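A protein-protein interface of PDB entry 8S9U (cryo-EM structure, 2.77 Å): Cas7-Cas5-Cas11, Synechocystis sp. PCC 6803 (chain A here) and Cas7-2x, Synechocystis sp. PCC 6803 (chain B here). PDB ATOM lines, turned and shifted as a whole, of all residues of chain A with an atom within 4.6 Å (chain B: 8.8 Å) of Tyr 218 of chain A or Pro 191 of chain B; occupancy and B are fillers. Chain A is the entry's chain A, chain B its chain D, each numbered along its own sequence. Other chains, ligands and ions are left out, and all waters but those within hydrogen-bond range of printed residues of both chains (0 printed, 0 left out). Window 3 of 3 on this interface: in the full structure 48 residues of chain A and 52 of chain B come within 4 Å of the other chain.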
ATOM      1  N   GLY A  58      15.218 -22.926 -16.249  1.00  0.00           N
ATOM      2  CA  GLY A  58      15.483 -21.860 -15.298  1.00  0.00           C
ATOM      3  C   GLY A  58      15.042 -20.499 -15.792  1.00  0.00           C
ATOM      4  O   GLY A  58      14.415 -19.735 -15.061  1.00  0.00           O
ATOM      5  N   LEU A  59      15.368 -20.173 -17.037  1.00  0.00           N
ATOM      6  CA  LEU A  59      14.951 -18.898 -17.607  1.00  0.00           C
ATOM      7  C   LEU A  59      13.442 -18.785 -17.734  1.00  0.00           C
ATOM      8  O   LEU A  59      12.905 -17.675 -17.695  1.00  0.00           O
ATOM      9  CB  LEU A  59      15.617 -18.690 -18.959  1.00  0.00           C
ATOM     10  CG  LEU A  59      17.134 -18.612 -18.905  1.00  0.00           C
ATOM     11  CD1 LEU A  59      17.701 -18.526 -20.281  1.00  0.00           C
ATOM     12  CD2 LEU A  59      17.513 -17.409 -18.128  1.00  0.00           C
ATOM     13  N   ASN A  61      11.497 -19.678 -15.480  1.00  0.00           N
ATOM     14  CA  ASN A  61      11.022 -19.732 -14.099  1.00  0.00           C
ATOM     15  C   ASN A  61      10.340 -21.064 -13.799  1.00  0.00           C
ATOM     16  O   ASN A  61       9.323 -21.117 -13.107  1.00  0.00           O
ATOM     17  CB  ASN A  61      10.094 -18.564 -13.775  1.00  0.00           C
ATOM     18  CG  ASN A  61      10.745 -17.232 -14.000  1.00  0.00           C
ATOM     19  OD1 ASN A  61      10.748 -16.715 -15.109  1.00  0.00           O
ATOM     20  ND2 ASN A  61      11.309 -16.666 -12.947  1.00  0.00           N
ATOM     21  N   TRP A  68      11.488 -19.902 -23.621  1.00  0.00           N
ATOM     22  CA  TRP A  68      12.818 -20.471 -23.767  1.00  0.00           C
ATOM     23  C   TRP A  68      12.815 -21.952 -24.095  1.00  0.00           C
ATOM     24  O   TRP A  68      13.771 -22.439 -24.699  1.00  0.00           O
ATOM     25  CB  TRP A  68      13.640 -20.207 -22.517  1.00  0.00           C
ATOM     26  CG  TRP A  68      13.914 -18.767 -22.364  1.00  0.00           C
ATOM     27  CD1 TRP A  68      13.173 -17.867 -21.684  1.00  0.00           C
ATOM     28  CD2 TRP A  68      14.942 -18.029 -23.017  1.00  0.00           C
ATOM     29  NE1 TRP A  68      13.712 -16.621 -21.809  1.00  0.00           N
ATOM     30  CE2 TRP A  68      14.799 -16.694 -22.634  1.00  0.00           C
ATOM     31  CE3 TRP A  68      15.989 -18.376 -23.869  1.00  0.00           C
ATOM     32  CZ2 TRP A  68      15.657 -15.703 -23.072  1.00  0.00           C
ATOM     33  CZ3 TRP A  68      16.838 -17.397 -24.298  1.00  0.00           C
ATOM     34  CH2 TRP A  68      16.670 -16.076 -23.903  1.00  0.00           C
ATOM     35  N   LEU A 214      23.627 -13.264 -22.639  1.00  0.00           N
ATOM     36  CA  LEU A 214      22.296 -13.772 -22.327  1.00  0.00           C
ATOM     37  C   LEU A 214      21.807 -13.264 -20.980  1.00  0.00           C
ATOM     38  O   LEU A 214      20.644 -12.881 -20.837  1.00  0.00           O
ATOM     39  CB  LEU A 214      22.305 -15.299 -22.364  1.00  0.00           C
ATOM     40  CG  LEU A 214      20.962 -15.994 -22.536  1.00  0.00           C
ATOM     41  CD1 LEU A 214      20.545 -15.931 -23.962  1.00  0.00           C
ATOM     42  CD2 LEU A 214      21.061 -17.418 -22.080  1.00  0.00           C
ATOM     43  N   LYS A 215      22.684 -13.258 -19.981  1.00  0.00           N
ATOM     44  CA  LYS A 215      22.344 -12.696 -18.681  1.00  0.00           C
ATOM     45  C   LYS A 215      21.896 -11.247 -18.789  1.00  0.00           C
ATOM     46  O   LYS A 215      20.927 -10.839 -18.142  1.00  0.00           O
ATOM     47  CB  LYS A 215      23.546 -12.822 -17.756  1.00  0.00           C
ATOM     48  CG  LYS A 215      23.313 -12.397 -16.344  1.00  0.00           C
ATOM     49  CD  LYS A 215      24.574 -12.611 -15.546  1.00  0.00           C
ATOM     50  CE  LYS A 215      24.357 -12.362 -14.080  1.00  0.00           C
ATOM     51  NZ  LYS A 215      24.177 -10.913 -13.833  1.00  0.00           N
ATOM     52  N   ASP A 216      22.593 -10.449 -19.590  1.00  0.00           N
ATOM     53  CA  ASP A 216      22.214  -9.057 -19.769  1.00  0.00           C
ATOM     54  C   ASP A 216      20.963  -8.876 -20.619  1.00  0.00           C
ATOM     55  O   ASP A 216      20.307  -7.837 -20.506  1.00  0.00           O
ATOM     56  CB  ASP A 216      23.370  -8.293 -20.398  1.00  0.00           C
ATOM     57  CG  ASP A 216      24.569  -8.213 -19.489  1.00  0.00           C
ATOM     58  OD1 ASP A 216      24.390  -8.330 -18.264  1.00  0.00           O
ATOM     59  OD2 ASP A 216      25.693  -8.041 -19.995  1.00  0.00           O
ATOM     60  N   ASN A 217      20.608  -9.848 -21.458  1.00  0.00           N
ATOM     61  CA  ASN A 217      19.591  -9.633 -22.478  1.00  0.00           C
ATOM     62  C   ASN A 217      18.422 -10.606 -22.491  1.00  0.00           C
ATOM     63  O   ASN A 217      17.493 -10.386 -23.269  1.00  0.00           O
ATOM     64  CB  ASN A 217      20.235  -9.655 -23.867  1.00  0.00           C
ATOM     65  CG  ASN A 217      21.141  -8.479 -24.100  1.00  0.00           C
ATOM     66  OD1 ASN A 217      20.709  -7.434 -24.573  1.00  0.00           O
ATOM     67  ND2 ASN A 217      22.407  -8.634 -23.753  1.00  0.00           N
ATOM     68  N   TYR A 218      18.441 -11.678 -21.699  1.00  0.00           N
ATOM     69  CA  TYR A 218      17.403 -12.700 -21.812  1.00  0.00           C
ATOM     70  C   TYR A 218      15.988 -12.151 -21.662  1.00  0.00           C
ATOM     71  O   TYR A 218      15.048 -12.719 -22.222  1.00  0.00           O
ATOM     72  CB  TYR A 218      17.640 -13.812 -20.792  1.00  0.00           C
ATOM     73  CG  TYR A 218      17.212 -13.483 -19.390  1.00  0.00           C
ATOM     74  CD1 TYR A 218      18.017 -12.723 -18.563  1.00  0.00           C
ATOM     75  CD2 TYR A 218      16.000 -13.921 -18.896  1.00  0.00           C
ATOM     76  CE1 TYR A 218      17.640 -12.427 -17.284  1.00  0.00           C
ATOM     77  CE2 TYR A 218      15.609 -13.616 -17.625  1.00  0.00           C
ATOM     78  CZ  TYR A 218      16.434 -12.871 -16.820  1.00  0.00           C
ATOM     79  OH  TYR A 218      16.040 -12.554 -15.547  1.00  0.00           O
ATOM     80  N   GLN A 219      15.805 -11.059 -20.928  1.00  0.00           N
ATOM     81  CA  GLN A 219      14.466 -10.502 -20.762  1.00  0.00           C
ATOM     82  C   GLN A 219      13.915  -9.852 -22.024  1.00  0.00           C
ATOM     83  O   GLN A 219      12.703  -9.641 -22.114  1.00  0.00           O
ATOM     84  CB  GLN A 219      14.475  -9.486 -19.628  1.00  0.00           C
ATOM     85  CG  GLN A 219      14.841 -10.078 -18.290  1.00  0.00           C
ATOM     86  CD  GLN A 219      14.966  -9.028 -17.215  1.00  0.00           C
ATOM     87  OE1 GLN A 219      14.489  -7.907 -17.371  1.00  0.00           O
ATOM     88  NE2 GLN A 219      15.619  -9.379 -16.119  1.00  0.00           N
ATOM     89  N   SER A 220      14.762  -9.529 -22.990  1.00  0.00           N
ATOM     90  CA  SER A 220      14.357  -8.849 -24.214  1.00  0.00           C
ATOM     91  C   SER A 220      14.027  -9.795 -25.362  1.00  0.00           C
ATOM     92  O   SER A 220      13.732  -9.322 -26.462  1.00  0.00           O
ATOM     93  CB  SER A 220      15.446  -7.871 -24.655  1.00  0.00           C
ATOM     94  OG  SER A 220      16.542  -8.554 -25.227  1.00  0.00           O
ATOM     95  N   VAL A 221      14.067 -11.104 -25.149  1.00  0.00           N
ATOM     96  CA  VAL A 221      14.133 -12.078 -26.230  1.00  0.00           C
ATOM     97  C   VAL A 221      12.730 -12.553 -26.576  1.00  0.00           C
ATOM     98  O   VAL A 221      11.973 -12.977 -25.698  1.00  0.00           O
ATOM     99  CB  VAL A 221      15.025 -13.264 -25.830  1.00  0.00           C
ATOM    100  CG1 VAL A 221      14.929 -14.369 -26.847  1.00  0.00           C
ATOM    101  CG2 VAL A 221      16.449 -12.809 -25.665  1.00  0.00           C
ATOM    102  N   ALA B 187      19.670 -21.691  -7.375  1.00  0.00           N
ATOM    103  CA  ALA B 187      18.251 -21.742  -7.720  1.00  0.00           C
ATOM    104  C   ALA B 187      18.083 -21.956  -9.219  1.00  0.00           C
ATOM    105  O   ALA B 187      17.758 -21.042  -9.975  1.00  0.00           O
ATOM    106  CB  ALA B 187      17.546 -20.474  -7.272  1.00  0.00           C
ATOM    107  N   LEU B 188      18.313 -23.194  -9.658  1.00  0.00           N
ATOM    108  CA  LEU B 188      18.168 -23.517 -11.070  1.00  0.00           C
ATOM    109  C   LEU B 188      16.748 -23.353 -11.574  1.00  0.00           C
ATOM    110  O   LEU B 188      16.523 -23.474 -12.779  1.00  0.00           O
ATOM    111  CB  LEU B 188      18.632 -24.941 -11.352  1.00  0.00           C
ATOM    112  CG  LEU B 188      20.066 -25.332 -11.050  1.00  0.00           C
ATOM    113  CD1 LEU B 188      20.416 -26.556 -11.830  1.00  0.00           C
ATOM    114  CD2 LEU B 188      20.975 -24.207 -11.440  1.00  0.00           C
ATOM    115  N   ASP B 189      15.791 -23.117 -10.693  1.00  0.00           N
ATOM    116  CA  ASP B 189      14.416 -22.849 -11.078  1.00  0.00           C
ATOM    117  C   ASP B 189      14.194 -21.434 -11.586  1.00  0.00           C
ATOM    118  O   ASP B 189      13.104 -21.146 -12.080  1.00  0.00           O
ATOM    119  CB  ASP B 189      13.499 -23.112  -9.886  1.00  0.00           C
ATOM    120  CG  ASP B 189      12.203 -23.775 -10.288  1.00  0.00           C
ATOM    121  OD1 ASP B 189      12.190 -24.462 -11.336  1.00  0.00           O
ATOM    122  OD2 ASP B 189      11.200 -23.625  -9.558  1.00  0.00           O
ATOM    123  N   LYS B 190      15.176 -20.550 -11.484  1.00  0.00           N
ATOM    124  CA  LYS B 190      14.977 -19.130 -11.721  1.00  0.00           C
ATOM    125  C   LYS B 190      16.129 -18.576 -12.541  1.00  0.00           C
ATOM    126  O   LYS B 190      17.239 -19.116 -12.505  1.00  0.00           O
ATOM    127  CB  LYS B 190      14.877 -18.368 -10.396  1.00  0.00           C
ATOM    128  CG  LYS B 190      13.740 -18.820  -9.525  1.00  0.00           C
ATOM    129  CD  LYS B 190      13.624 -17.984  -8.277  1.00  0.00           C
ATOM    130  CE  LYS B 190      12.496 -18.493  -7.407  1.00  0.00           C
ATOM    131  NZ  LYS B 190      12.491 -17.837  -6.076  1.00  0.00           N
ATOM    132  N   PRO B 191      15.904 -17.476 -13.265  1.00  0.00           N
ATOM    133  CA  PRO B 191      16.977 -16.905 -14.092  1.00  0.00           C
ATOM    134  C   PRO B 191      18.231 -16.561 -13.325  1.00  0.00           C
ATOM    135  O   PRO B 191      19.335 -16.846 -13.794  1.00  0.00           O
ATOM    136  CB  PRO B 191      16.326 -15.654 -14.681  1.00  0.00           C
ATOM    137  CG  PRO B 191      14.905 -15.944 -14.684  1.00  0.00           C
ATOM    138  CD  PRO B 191      14.622 -16.795 -13.498  1.00  0.00           C
ATOM    139  N   GLU B 192      18.101 -15.934 -12.164  1.00  0.00           N
ATOM    140  CA  GLU B 192      19.282 -15.460 -11.457  1.00  0.00           C
ATOM    141  C   GLU B 192      20.107 -16.620 -10.931  1.00  0.00           C
ATOM    142  O   GLU B 192      21.338 -16.565 -10.926  1.00  0.00           O
ATOM    143  CB  GLU B 192      18.853 -14.540 -10.321  1.00  0.00           C
ATOM    144  CG  GLU B 192      17.970 -13.393 -10.791  1.00  0.00           C
ATOM    145  CD  GLU B 192      16.497 -13.772 -10.853  1.00  0.00           C
ATOM    146  OE1 GLU B 192      15.650 -12.869 -11.012  1.00  0.00           O
ATOM    147  OE2 GLU B 192      16.187 -14.972 -10.722  1.00  0.00           O
ATOM    148  N   GLY B 193      19.443 -17.680 -10.484  1.00  0.00           N
ATOM    149  CA  GLY B 193      20.143 -18.856 -10.013  1.00  0.00           C
ATOM    150  C   GLY B 193      20.737 -19.723 -11.094  1.00  0.00           C
ATOM    151  O   GLY B 193      21.735 -20.405 -10.857  1.00  0.00           O
ATOM    152  N   ILE B 194      20.120 -19.759 -12.272  1.00  0.00           N
ATOM    153  CA  ILE B 194      20.730 -20.484 -13.381  1.00  0.00           C
ATOM    154  C   ILE B 194      21.979 -19.763 -13.885  1.00  0.00           C
ATOM    155  O   ILE B 194      22.989 -20.400 -14.195  1.00  0.00           O
ATOM    156  CB  ILE B 194      19.701 -20.721 -14.503  1.00  0.00           C
ATOM    157  CG1 ILE B 194      20.244 -21.717 -15.501  1.00  0.00           C
ATOM    158  CG2 ILE B 194      19.407 -19.474 -15.272  1.00  0.00           C
ATOM    159  CD1 ILE B 194      20.407 -23.073 -14.917  1.00  0.00           C
ATOM    160  N   PHE B 195      21.945 -18.435 -13.971  1.00  0.00           N
ATOM    161  CA  PHE B 195      23.151 -17.693 -14.309  1.00  0.00           C
ATOM    162  C   PHE B 195      24.203 -17.765 -13.216  1.00  0.00           C
ATOM    163  O   PHE B 195      25.399 -17.776 -13.514  1.00  0.00           O
ATOM    164  CB  PHE B 195      22.790 -16.253 -14.628  1.00  0.00           C
ATOM    165  CG  PHE B 195      22.081 -16.110 -15.928  1.00  0.00           C
ATOM    166  CD1 PHE B 195      22.644 -16.598 -17.086  1.00  0.00           C
ATOM    167  CD2 PHE B 195      20.844 -15.520 -15.994  1.00  0.00           C
ATOM    168  CE1 PHE B 195      21.991 -16.490 -18.271  1.00  0.00           C
ATOM    169  CE2 PHE B 195      20.188 -15.414 -17.185  1.00  0.00           C
ATOM    170  CZ  PHE B 195      20.763 -15.895 -18.320  1.00  0.00           C
ATOM    171  N   SER B 196      23.788 -17.798 -11.952  1.00  0.00           N
ATOM    172  CA  SER B 196      24.732 -18.021 -10.864  1.00  0.00           C
ATOM    173  C   SER B 196      25.423 -19.368 -10.996  1.00  0.00           C
ATOM    174  O   SER B 196      26.600 -19.506 -10.657  1.00  0.00           O
ATOM    175  CB  SER B 196      24.016 -17.912  -9.526  1.00  0.00           C
ATOM    176  OG  SER B 196      24.915 -18.090  -8.452  1.00  0.00           O
ATOM    177  N   ALA B 197      24.700 -20.385 -11.457  1.00  0.00           N
ATOM    178  CA  ALA B 197      25.338 -21.664 -11.736  1.00  0.00           C
ATOM    179  C   ALA B 197      26.376 -21.522 -12.829  1.00  0.00           C
ATOM    180  O   ALA B 197      27.442 -22.144 -12.773  1.00  0.00           O
ATOM    181  CB  ALA B 197      24.294 -22.700 -12.133  1.00  0.00           C
ATOM    182  N   LEU B 198      26.073 -20.724 -13.842  1.00  0.00           N
ATOM    183  CA  LEU B 198      26.979 -20.544 -14.964  1.00  0.00           C
ATOM    184  C   LEU B 198      28.153 -19.646 -14.616  1.00  0.00           C
ATOM    185  O   LEU B 198      29.210 -19.762 -15.236  1.00  0.00           O
ATOM    186  CB  LEU B 198      26.207 -19.988 -16.156  1.00  0.00           C
ATOM    187  CG  LEU B 198      25.156 -20.985 -16.634  1.00  0.00           C
ATOM    188  CD1 LEU B 198      24.198 -20.341 -17.587  1.00  0.00           C
ATOM    189  CD2 LEU B 198      25.784 -22.199 -17.237  1.00  0.00           C
ATOM    190  N   LEU B 199      27.999 -18.736 -13.657  1.00  0.00           N
ATOM    191  CA  LEU B 199      28.982 -17.670 -13.529  1.00  0.00           C
ATOM    192  C   LEU B 199      29.448 -17.373 -12.101  1.00  0.00           C
ATOM    193  O   LEU B 199      30.633 -17.103 -11.894  1.00  0.00           O
ATOM    194  CB  LEU B 199      28.401 -16.395 -14.149  1.00  0.00           C
ATOM    195  CG  LEU B 199      28.103 -16.376 -15.651  1.00  0.00           C
ATOM    196  CD1 LEU B 199      27.268 -15.172 -16.016  1.00  0.00           C
ATOM    197  CD2 LEU B 199      29.363 -16.395 -16.484  1.00  0.00           C
ATOM    198  N   ASP B 200      28.556 -17.427 -11.108  1.00  0.00           N
ATOM    199  CA  ASP B 200      28.816 -16.821  -9.799  1.00  0.00           C
ATOM    200  C   ASP B 200      29.203 -17.783  -8.678  1.00  0.00           C
ATOM    201  O   ASP B 200      29.455 -17.320  -7.565  1.00  0.00           O
ATOM    202  CB  ASP B 200      27.601 -16.004  -9.352  1.00  0.00           C
ATOM    203  CG  ASP B 200      27.179 -14.979 -10.382  1.00  0.00           C
ATOM    204  OD1 ASP B 200      28.043 -14.545 -11.171  1.00  0.00           O
ATOM    205  OD2 ASP B 200      25.989 -14.602 -10.404  1.00  0.00           O
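The backbone nitrogen (N) of Pro 191 of chain B sits close to the backbone carbonyl oxygen (O) of Gly 58 of chain A, at 3.2 Å.
NE2 of Gln 219 of chain A sits at hydrogen-bond distance from OH of Tyr 218 of chain A (3.3 Å).
Among the printed residues, merely in contact across the chains: Gly 58 of chain A with Leu 188 of chain B (3.2 Å), Gly 58 of chain A with Asp 189 of chain B (3.5 Å), Gly 58 of chain A with Lys 190 of chain B (3.3 Å), Leu 59 of chain A with Phe 195 of chain B (3.5 Å), Asn 61 of chain A with Asp 189 of chain B (3.2 Å), Asn 61 of chain A with Pro 191 of chain B (3.4 Å), Leu 214 of chain A with Phe 195 of chain B (3.9 Å), Lys 215 of chain A with Phe 195 of chain B (3.6 Å), Lys 215 of chain A with Leu 199 of chain B (3.7 Å), Tyr 218 of chain A with Pro 191 of chain B (3.2 Å) and Tyr 218 of chain A with Phe 195 of chain B (3.7 Å).
Of the printed residues of chain B, Asn 61 of chain A touches Asp 189 (3.2 Å) and Pro 191 (3.4 Å). Printed residues of chain B within 4 Å of Leu 214 of chain A: Phe 195 (3.9 Å). Of the printed residues of chain B, Tyr 218 of chain A touches Pro 191 and Phe 195. Printed residues of chain A within 4 Å of Pro 191 of chain B: Gly 58 (3.2 Å), Asn 61 (3.4 Å) and Tyr 218 (3.2 Å). Ile 194 of chain B touches none of the printed residues of chain A. The nearest residue of chain B that does not touch Tyr 218 of chain A is Glu 192 of chain B (4.6 Å). The nearest printed residue of chain A that does not touch Leu 188 of chain B is Leu 59 of chain A (5.5 Å).
Printed residues of chain B that touch a printed residue of chain A: Leu 188, Asp 189, Lys 190, Pro 191, Phe 195 and Leu 199. Hydrophobic or aromatic side chains of chain B within 4 Å of the printed part of chain A: Pro 191, Phe 195 and Leu 199. Among the printed residues, 12 pairs touch across the chains. Among the printed residues, no Asp or Glu carboxylate lies within 4 Å of a Lys or Arg side-chain nitrogen of the other chain.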
